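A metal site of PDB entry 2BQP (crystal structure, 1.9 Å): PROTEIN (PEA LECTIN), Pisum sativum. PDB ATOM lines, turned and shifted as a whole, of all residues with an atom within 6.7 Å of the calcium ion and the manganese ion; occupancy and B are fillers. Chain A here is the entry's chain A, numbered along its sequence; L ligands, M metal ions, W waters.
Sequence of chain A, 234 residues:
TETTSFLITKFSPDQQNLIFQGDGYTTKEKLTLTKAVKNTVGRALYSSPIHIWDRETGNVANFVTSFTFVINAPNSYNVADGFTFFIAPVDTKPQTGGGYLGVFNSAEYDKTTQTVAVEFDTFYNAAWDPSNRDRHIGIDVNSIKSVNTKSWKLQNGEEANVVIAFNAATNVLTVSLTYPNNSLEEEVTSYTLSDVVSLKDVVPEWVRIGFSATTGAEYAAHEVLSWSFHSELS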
ATOM      1  N   ASP A  81       4.402  11.525  28.962  1.00  0.00           N
ATOM      2  CA  ASP A  81       4.854  11.137  27.629  1.00  0.00           C
ATOM      3  C   ASP A  81       5.487  12.273  26.836  1.00  0.00           C
ATOM      4  O   ASP A  81       6.254  12.033  25.890  1.00  0.00           O
ATOM      5  CB  ASP A  81       3.688  10.598  26.826  1.00  0.00           C
ATOM      6  CG  ASP A  81       3.519   9.116  26.983  1.00  0.00           C
ATOM      7  OD1 ASP A  81       4.261   8.408  26.291  1.00  0.00           O
ATOM      8  OD2 ASP A  81       2.682   8.676  27.796  1.00  0.00           O
ATOM      9  N   GLY A  99       1.550   7.776  24.164  1.00  0.00           N
ATOM     10  CA  GLY A  99       2.650   8.007  23.245  1.00  0.00           C
ATOM     11  C   GLY A  99       2.307   8.807  22.024  1.00  0.00           C
ATOM     12  O   GLY A  99       3.206   9.332  21.392  1.00  0.00           O
ATOM     13  N   TYR A 100       1.024   8.900  21.687  1.00  0.00           N
ATOM     14  CA  TYR A 100       0.566   9.691  20.536  1.00  0.00           C
ATOM     15  C   TYR A 100       0.454  11.191  20.853  1.00  0.00           C
ATOM     16  O   TYR A 100       0.193  12.013  19.971  1.00  0.00           O
ATOM     17  CB  TYR A 100      -0.761   9.141  20.016  1.00  0.00           C
ATOM     18  CG  TYR A 100      -0.581   7.805  19.356  1.00  0.00           C
ATOM     19  CD1 TYR A 100      -0.197   7.723  18.017  1.00  0.00           C
ATOM     20  CD2 TYR A 100      -0.737   6.635  20.075  1.00  0.00           C
ATOM     21  CE1 TYR A 100       0.049   6.484  17.425  1.00  0.00           C
ATOM     22  CE2 TYR A 100      -0.500   5.399  19.494  1.00  0.00           C
ATOM     23  CZ  TYR A 100      -0.112   5.333  18.172  1.00  0.00           C
ATOM     24  OH  TYR A 100       0.112   4.096  17.590  1.00  0.00           O
ATOM     25  N   LEU A 101       0.637  11.526  22.129  1.00  0.00           N
ATOM     26  CA  LEU A 101       0.667  12.899  22.613  1.00  0.00           C
ATOM     27  C   LEU A 101      -0.592  13.718  22.394  1.00  0.00           C
ATOM     28  O   LEU A 101      -0.541  14.954  22.433  1.00  0.00           O
ATOM     29  CB  LEU A 101       1.907  13.609  22.029  1.00  0.00           C
ATOM     30  CG  LEU A 101       3.244  12.941  22.358  1.00  0.00           C
ATOM     31  CD1 LEU A 101       4.364  13.553  21.503  1.00  0.00           C
ATOM     32  CD2 LEU A 101       3.533  13.071  23.835  1.00  0.00           C
ATOM     33  N   GLU A 119       7.455  18.150  18.825  1.00  0.00           N
ATOM     34  CA  GLU A 119       7.384  17.416  20.078  1.00  0.00           C
ATOM     35  C   GLU A 119       8.584  17.449  20.993  1.00  0.00           C
ATOM     36  O   GLU A 119       9.727  17.603  20.546  1.00  0.00           O
ATOM     37  CB  GLU A 119       7.024  15.968  19.810  1.00  0.00           C
ATOM     38  CG  GLU A 119       8.124  15.213  19.017  1.00  0.00           C
ATOM     39  CD  GLU A 119       7.930  13.703  19.014  1.00  0.00           C
ATOM     40  OE1 GLU A 119       6.947  13.235  18.409  1.00  0.00           O
ATOM     41  OE2 GLU A 119       8.767  12.999  19.624  1.00  0.00           O
ATOM     42  N   ASP A 121       9.408  14.838  23.384  1.00  0.00           N
ATOM     43  CA  ASP A 121       9.075  13.481  23.724  1.00  0.00           C
ATOM     44  C   ASP A 121       9.957  12.948  24.834  1.00  0.00           C
ATOM     45  O   ASP A 121      11.166  12.771  24.649  1.00  0.00           O
ATOM     46  CB  ASP A 121       9.236  12.670  22.436  1.00  0.00           C
ATOM     47  CG  ASP A 121       8.711  11.278  22.538  1.00  0.00           C
ATOM     48  OD1 ASP A 121       8.513  10.779  23.664  1.00  0.00           O
ATOM     49  OD2 ASP A 121       8.565  10.649  21.454  1.00  0.00           O
ATOM     50  N   THR A 122       9.340  12.579  25.941  1.00  0.00           N
ATOM     51  CA  THR A 122      10.073  12.083  27.106  1.00  0.00           C
ATOM     52  C   THR A 122      10.060  10.574  27.350  1.00  0.00           C
ATOM     53  O   THR A 122      10.619  10.111  28.345  1.00  0.00           O
ATOM     54  CB  THR A 122       9.538  12.737  28.387  1.00  0.00           C
ATOM     55  OG1 THR A 122       8.135  12.491  28.501  1.00  0.00           O
ATOM     56  CG2 THR A 122       9.770  14.237  28.365  1.00  0.00           C
ATOM     57  N   PHE A 123       9.434   9.811  26.468  1.00  0.00           N
ATOM     58  CA  PHE A 123       9.323   8.372  26.673  1.00  0.00           C
ATOM     59  C   PHE A 123       9.511   7.638  25.371  1.00  0.00           C
ATOM     60  O   PHE A 123       8.837   7.914  24.370  1.00  0.00           O
ATOM     61  CB  PHE A 123       7.950   8.051  27.249  1.00  0.00           C
ATOM     62  CG  PHE A 123       7.679   6.575  27.440  1.00  0.00           C
ATOM     63  CD1 PHE A 123       8.034   5.944  28.617  1.00  0.00           C
ATOM     64  CD2 PHE A 123       7.040   5.849  26.454  1.00  0.00           C
ATOM     65  CE1 PHE A 123       7.747   4.614  28.818  1.00  0.00           C
ATOM     66  CE2 PHE A 123       6.747   4.515  26.643  1.00  0.00           C
ATOM     67  CZ  PHE A 123       7.101   3.894  27.835  1.00  0.00           C
ATOM     68  N   TYR A 124      10.379   6.627  25.420  1.00  0.00           N
ATOM     69  CA  TYR A 124      10.718   5.824  24.253  1.00  0.00           C
ATOM     70  C   TYR A 124       9.632   4.833  23.860  1.00  0.00           C
ATOM     71  O   TYR A 124       9.297   3.964  24.646  1.00  0.00           O
ATOM     72  CB  TYR A 124      12.036   5.095  24.537  1.00  0.00           C
ATOM     73  CG  TYR A 124      12.392   4.087  23.476  1.00  0.00           C
ATOM     74  CD1 TYR A 124      12.637   4.492  22.167  1.00  0.00           C
ATOM     75  CD2 TYR A 124      12.481   2.726  23.786  1.00  0.00           C
ATOM     76  CE1 TYR A 124      12.947   3.556  21.164  1.00  0.00           C
ATOM     77  CE2 TYR A 124      12.791   1.787  22.792  1.00  0.00           C
ATOM     78  CZ  TYR A 124      13.026   2.214  21.481  1.00  0.00           C
ATOM     79  OH  TYR A 124      13.335   1.292  20.483  1.00  0.00           O
ATOM     80  N   ASN A 125       9.033   5.015  22.687  1.00  0.00           N
ATOM     81  CA  ASN A 125       8.001   4.101  22.184  1.00  0.00           C
ATOM     82  C   ASN A 125       8.722   3.358  21.084  1.00  0.00           C
ATOM     83  O   ASN A 125       8.921   3.900  19.985  1.00  0.00           O
ATOM     84  CB  ASN A 125       6.778   4.810  21.595  1.00  0.00           C
ATOM     85  CG  ASN A 125       5.987   5.566  22.635  1.00  0.00           C
ATOM     86  OD1 ASN A 125       6.151   6.766  22.769  1.00  0.00           O
ATOM     87  ND2 ASN A 125       5.208   4.854  23.423  1.00  0.00           N
ATOM     88  N   TRP A 128       8.211   3.399  17.100  1.00  0.00           N
ATOM     89  CA  TRP A 128       8.516   4.524  16.206  1.00  0.00           C
ATOM     90  C   TRP A 128       9.590   5.530  16.657  1.00  0.00           C
ATOM     91  O   TRP A 128      10.080   6.299  15.825  1.00  0.00           O
ATOM     92  CB  TRP A 128       7.237   5.319  15.839  1.00  0.00           C
ATOM     93  CG  TRP A 128       6.572   5.959  17.051  1.00  0.00           C
ATOM     94  CD1 TRP A 128       7.013   7.052  17.755  1.00  0.00           C
ATOM     95  CD2 TRP A 128       5.425   5.470  17.748  1.00  0.00           C
ATOM     96  NE1 TRP A 128       6.222   7.262  18.839  1.00  0.00           N
ATOM     97  CE2 TRP A 128       5.240   6.311  18.866  1.00  0.00           C
ATOM     98  CE3 TRP A 128       4.544   4.415  17.535  1.00  0.00           C
ATOM     99  CZ2 TRP A 128       4.208   6.120  19.780  1.00  0.00           C
ATOM    100  CZ3 TRP A 128       3.527   4.220  18.426  1.00  0.00           C
ATOM    101  CH2 TRP A 128       3.355   5.075  19.549  1.00  0.00           C
ATOM    102  N   ASP A 129       9.896   5.577  17.955  1.00  0.00           N
ATOM    103  CA  ASP A 129      10.873   6.546  18.436  1.00  0.00           C
ATOM    104  C   ASP A 129      12.314   6.144  18.074  1.00  0.00           C
ATOM    105  O   ASP A 129      12.548   4.990  17.682  1.00  0.00           O
ATOM    106  CB  ASP A 129      10.742   6.718  19.947  1.00  0.00           C
ATOM    107  CG  ASP A 129       9.575   7.614  20.333  1.00  0.00           C
ATOM    108  OD1 ASP A 129       9.204   8.501  19.527  1.00  0.00           O
ATOM    109  OD2 ASP A 129       9.030   7.444  21.439  1.00  0.00           O
ATOM    110  N   PRO A 130      13.262   7.101  18.144  1.00  0.00           N
ATOM    111  CA  PRO A 130      14.677   6.850  17.838  1.00  0.00           C
ATOM    112  C   PRO A 130      15.246   5.653  18.626  1.00  0.00           C
ATOM    113  O   PRO A 130      15.083   5.576  19.854  1.00  0.00           O
ATOM    114  CB  PRO A 130      15.351   8.149  18.267  1.00  0.00           C
ATOM    115  CG  PRO A 130      14.362   9.152  17.926  1.00  0.00           C
ATOM    116  CD  PRO A 130      13.067   8.535  18.426  1.00  0.00           C
ATOM    117  N   HIS A 136      13.902  13.286  23.099  1.00  0.00           N
ATOM    118  CA  HIS A 136      14.274  14.088  21.968  1.00  0.00           C
ATOM    119  C   HIS A 136      13.257  15.162  21.611  1.00  0.00           C
ATOM    120  O   HIS A 136      12.113  15.135  22.084  1.00  0.00           O
ATOM    121  CB  HIS A 136      14.445  13.139  20.768  1.00  0.00           C
ATOM    122  CG  HIS A 136      13.318  12.158  20.623  1.00  0.00           C
ATOM    123  ND1 HIS A 136      13.105  11.114  21.495  1.00  0.00           N
ATOM    124  CD2 HIS A 136      12.288  12.120  19.739  1.00  0.00           C
ATOM    125  CE1 HIS A 136      12.006  10.476  21.168  1.00  0.00           C
ATOM    126  NE2 HIS A 136      11.488  11.058  20.089  1.00  0.00           N
ATOM    127  N   GLY A 138      11.459  16.719  18.229  1.00  0.00           N
ATOM    128  CA  GLY A 138      11.199  16.195  16.905  1.00  0.00           C
ATOM    129  C   GLY A 138      10.178  17.004  16.173  1.00  0.00           C
ATOM    130  O   GLY A 138       9.395  17.739  16.779  1.00  0.00           O
ATOM    131  N   ASP A 140       7.097  16.647  13.709  1.00  0.00           N
ATOM    132  CA  ASP A 140       6.112  15.694  13.203  1.00  0.00           C
ATOM    133  C   ASP A 140       5.199  16.304  12.142  1.00  0.00           C
ATOM    134  O   ASP A 140       4.764  17.460  12.256  1.00  0.00           O
ATOM    135  CB  ASP A 140       5.274  15.177  14.371  1.00  0.00           C
ATOM    136  CG  ASP A 140       6.113  14.629  15.507  1.00  0.00           C
ATOM    137  OD1 ASP A 140       7.305  14.350  15.305  1.00  0.00           O
ATOM    138  OD2 ASP A 140       5.590  14.451  16.620  1.00  0.00           O
ATOM    139  N   ILE A 144       3.177  10.324  14.138  1.00  0.00           N
ATOM    140  CA  ILE A 144       3.889  10.444  15.412  1.00  0.00           C
ATOM    141  C   ILE A 144       5.375  10.070  15.241  1.00  0.00           C
ATOM    142  O   ILE A 144       6.181  10.251  16.177  1.00  0.00           O
ATOM    143  CB  ILE A 144       3.231   9.585  16.541  1.00  0.00           C
ATOM    144  CG1 ILE A 144       3.777  10.008  17.925  1.00  0.00           C
ATOM    145  CG2 ILE A 144       3.493   8.096  16.325  1.00  0.00           C
ATOM    146  CD1 ILE A 144       3.536  11.494  18.321  1.00  0.00           C
ATOM    147  N   LYS A 145       5.721   9.532  14.076  1.00  0.00           N
ATOM    148  CA  LYS A 145       7.117   9.175  13.805  1.00  0.00           C
ATOM    149  C   LYS A 145       7.711  10.425  13.161  1.00  0.00           C
ATOM    150  O   LYS A 145       7.419  10.721  12.010  1.00  0.00           O
ATOM    151  CB  LYS A 145       7.195   8.003  12.831  1.00  0.00           C
ATOM    152  CG  LYS A 145       8.550   7.334  12.796  1.00  0.00           C
ATOM    153  CD  LYS A 145       8.657   6.375  11.624  1.00  0.00           C
ATOM    154  CE  LYS A 145       9.911   5.520  11.733  1.00  0.00           C
ATOM    155  NZ  LYS A 145       9.800   4.541  12.853  1.00  0.00           N
ATOM    156  N   SER A 146       8.501  11.156  13.936  1.00  0.00           N
ATOM    157  CA  SER A 146       9.113  12.410  13.496  1.00  0.00           C
ATOM    158  C   SER A 146       9.885  12.342  12.186  1.00  0.00           C
ATOM    159  O   SER A 146      10.445  11.313  11.854  1.00  0.00           O
ATOM    160  CB  SER A 146      10.046  12.929  14.588  1.00  0.00           C
ATOM    161  OG  SER A 146       9.470  12.770  15.879  1.00  0.00           O
ATOM    162  N   THR A 149      14.679  14.354  14.397  1.00  0.00           N
ATOM    163  CA  THR A 149      14.680  14.447  15.859  1.00  0.00           C
ATOM    164  C   THR A 149      16.065  14.870  16.333  1.00  0.00           C
ATOM    165  O   THR A 149      17.015  14.849  15.554  1.00  0.00           O
ATOM    166  CB  THR A 149      14.345  13.104  16.535  1.00  0.00           C
ATOM    167  OG1 THR A 149      15.422  12.172  16.338  1.00  0.00           O
ATOM    168  CG2 THR A 149      13.076  12.504  15.943  1.00  0.00           C
HETATM  169  C1  LIG L   1       1.482   3.024  27.893  1.00  0.00           C
HETATM  170  C2  LIG L   1       0.816   3.645  26.678  1.00  0.00           C
HETATM  171  C3  LIG L   1       1.885   4.278  25.810  1.00  0.00           C
HETATM  172  C4  LIG L   1       2.686   5.288  26.613  1.00  0.00           C
HETATM  173  C5  LIG L   1       3.249   4.619  27.863  1.00  0.00           C
HETATM  174  C6  LIG L   1       4.017   5.557  28.788  1.00  0.00           C
HETATM  175  O1  LIG L   1       0.523   2.457  28.701  1.00  0.00           O
HETATM  176  O2  LIG L   1       0.117   2.638  25.962  1.00  0.00           O
HETATM  177  O3  LIG L   1       1.295   4.943  24.708  1.00  0.00           O
HETATM  178  O4  LIG L   1       3.739   5.775  25.809  1.00  0.00           O
HETATM  179  O5  LIG L   1       2.179   4.037  28.632  1.00  0.00           O
HETATM  180  O6  LIG L   1       3.145   6.398  29.529  1.00  0.00           O
HETATM  181 CA    CA M   1       7.522   8.732  22.894  1.00  0.00          CA
HETATM  182 MN    MN M   2       9.079  10.737  19.508  1.00  0.00          MN
HETATM  183  O   HOH W   1       6.128   9.100  21.379  1.00  0.00           O
HETATM  184  O   HOH W   2       9.753  10.980  17.918  1.00  0.00           O
HETATM  185  O   HOH W   3       7.151  10.612  18.703  1.00  0.00           O
HETATM  186  O   HOH W   4       6.244   9.534  24.512  1.00  0.00           O
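Water W1 lies within hydrogen-bond range of the backbone carbonyl oxygen (O) of Gly 99 and the indole nitrogen (NE1) of Trp 128.
Water W3 lies within hydrogen-bond range of OE1 of Glu 119 (2.6 Å), O of Ile 144 (2.7 Å) and NE1 of Trp 128 (3.5 Å).
The manganese ion is bound by water W2 (1.7 Å).
The manganese ion is bound by OD2 of Asp 121, at 2.0 Å.
Water W3 is bound to the manganese ion.
OD1 of Asp 129 binds the manganese ion, 2.2 Å away.
The manganese ion is bound by the side-chain carboxylate (OE2) of Glu 119 (2.3 Å).
NE2 of His 136 is bound to the manganese ion (2.5 Å).
Within 4 Å of the manganese ion: Glu 119, Asp 121, Asp 129 and His 136.
The nearest printed residue that does not touch the manganese ion is Ser 146 (4.2 Å).
The side-chain carboxylate of Asp 129 lies close to the indole nitrogen of Trp 128, at 3.3 Å.
OE1 of Glu 119 sits close to OD2 of Asp 140 (2.6 Å).
The backbone carbonyl oxygen (O) of Gly 138 lies within hydrogen-bond range of the backbone NH (N) of Glu 119 (2.8 Å).
ND2 of Asn 125 sits at hydrogen-bond distance from O4 of the ligand.
The backbone NH (N) of Gly 99 sits at hydrogen-bond distance from an oxygen (O3) of the ligand.
The side-chain carboxylate (OD1) of Asp 81 lies within hydrogen-bond range of an oxygen (O4) of the ligand, at 2.7 Å.
The nearest printed residue that does not touch the calcium ion is Tyr 124 (4.4 Å).
The calcium ion is bound by water W1 (2.1 Å), O of Phe 123 (2.1 Å), water W4 (2.2 Å), OD1 of Asn 125 (2.4 Å), OD1 of Asp 121 (2.4 Å), OD2 of Asp 129 (2.5 Å) and OD2 of Asp 121 (2.6 Å).
The calcium ion has seven donor atoms within binding distance.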
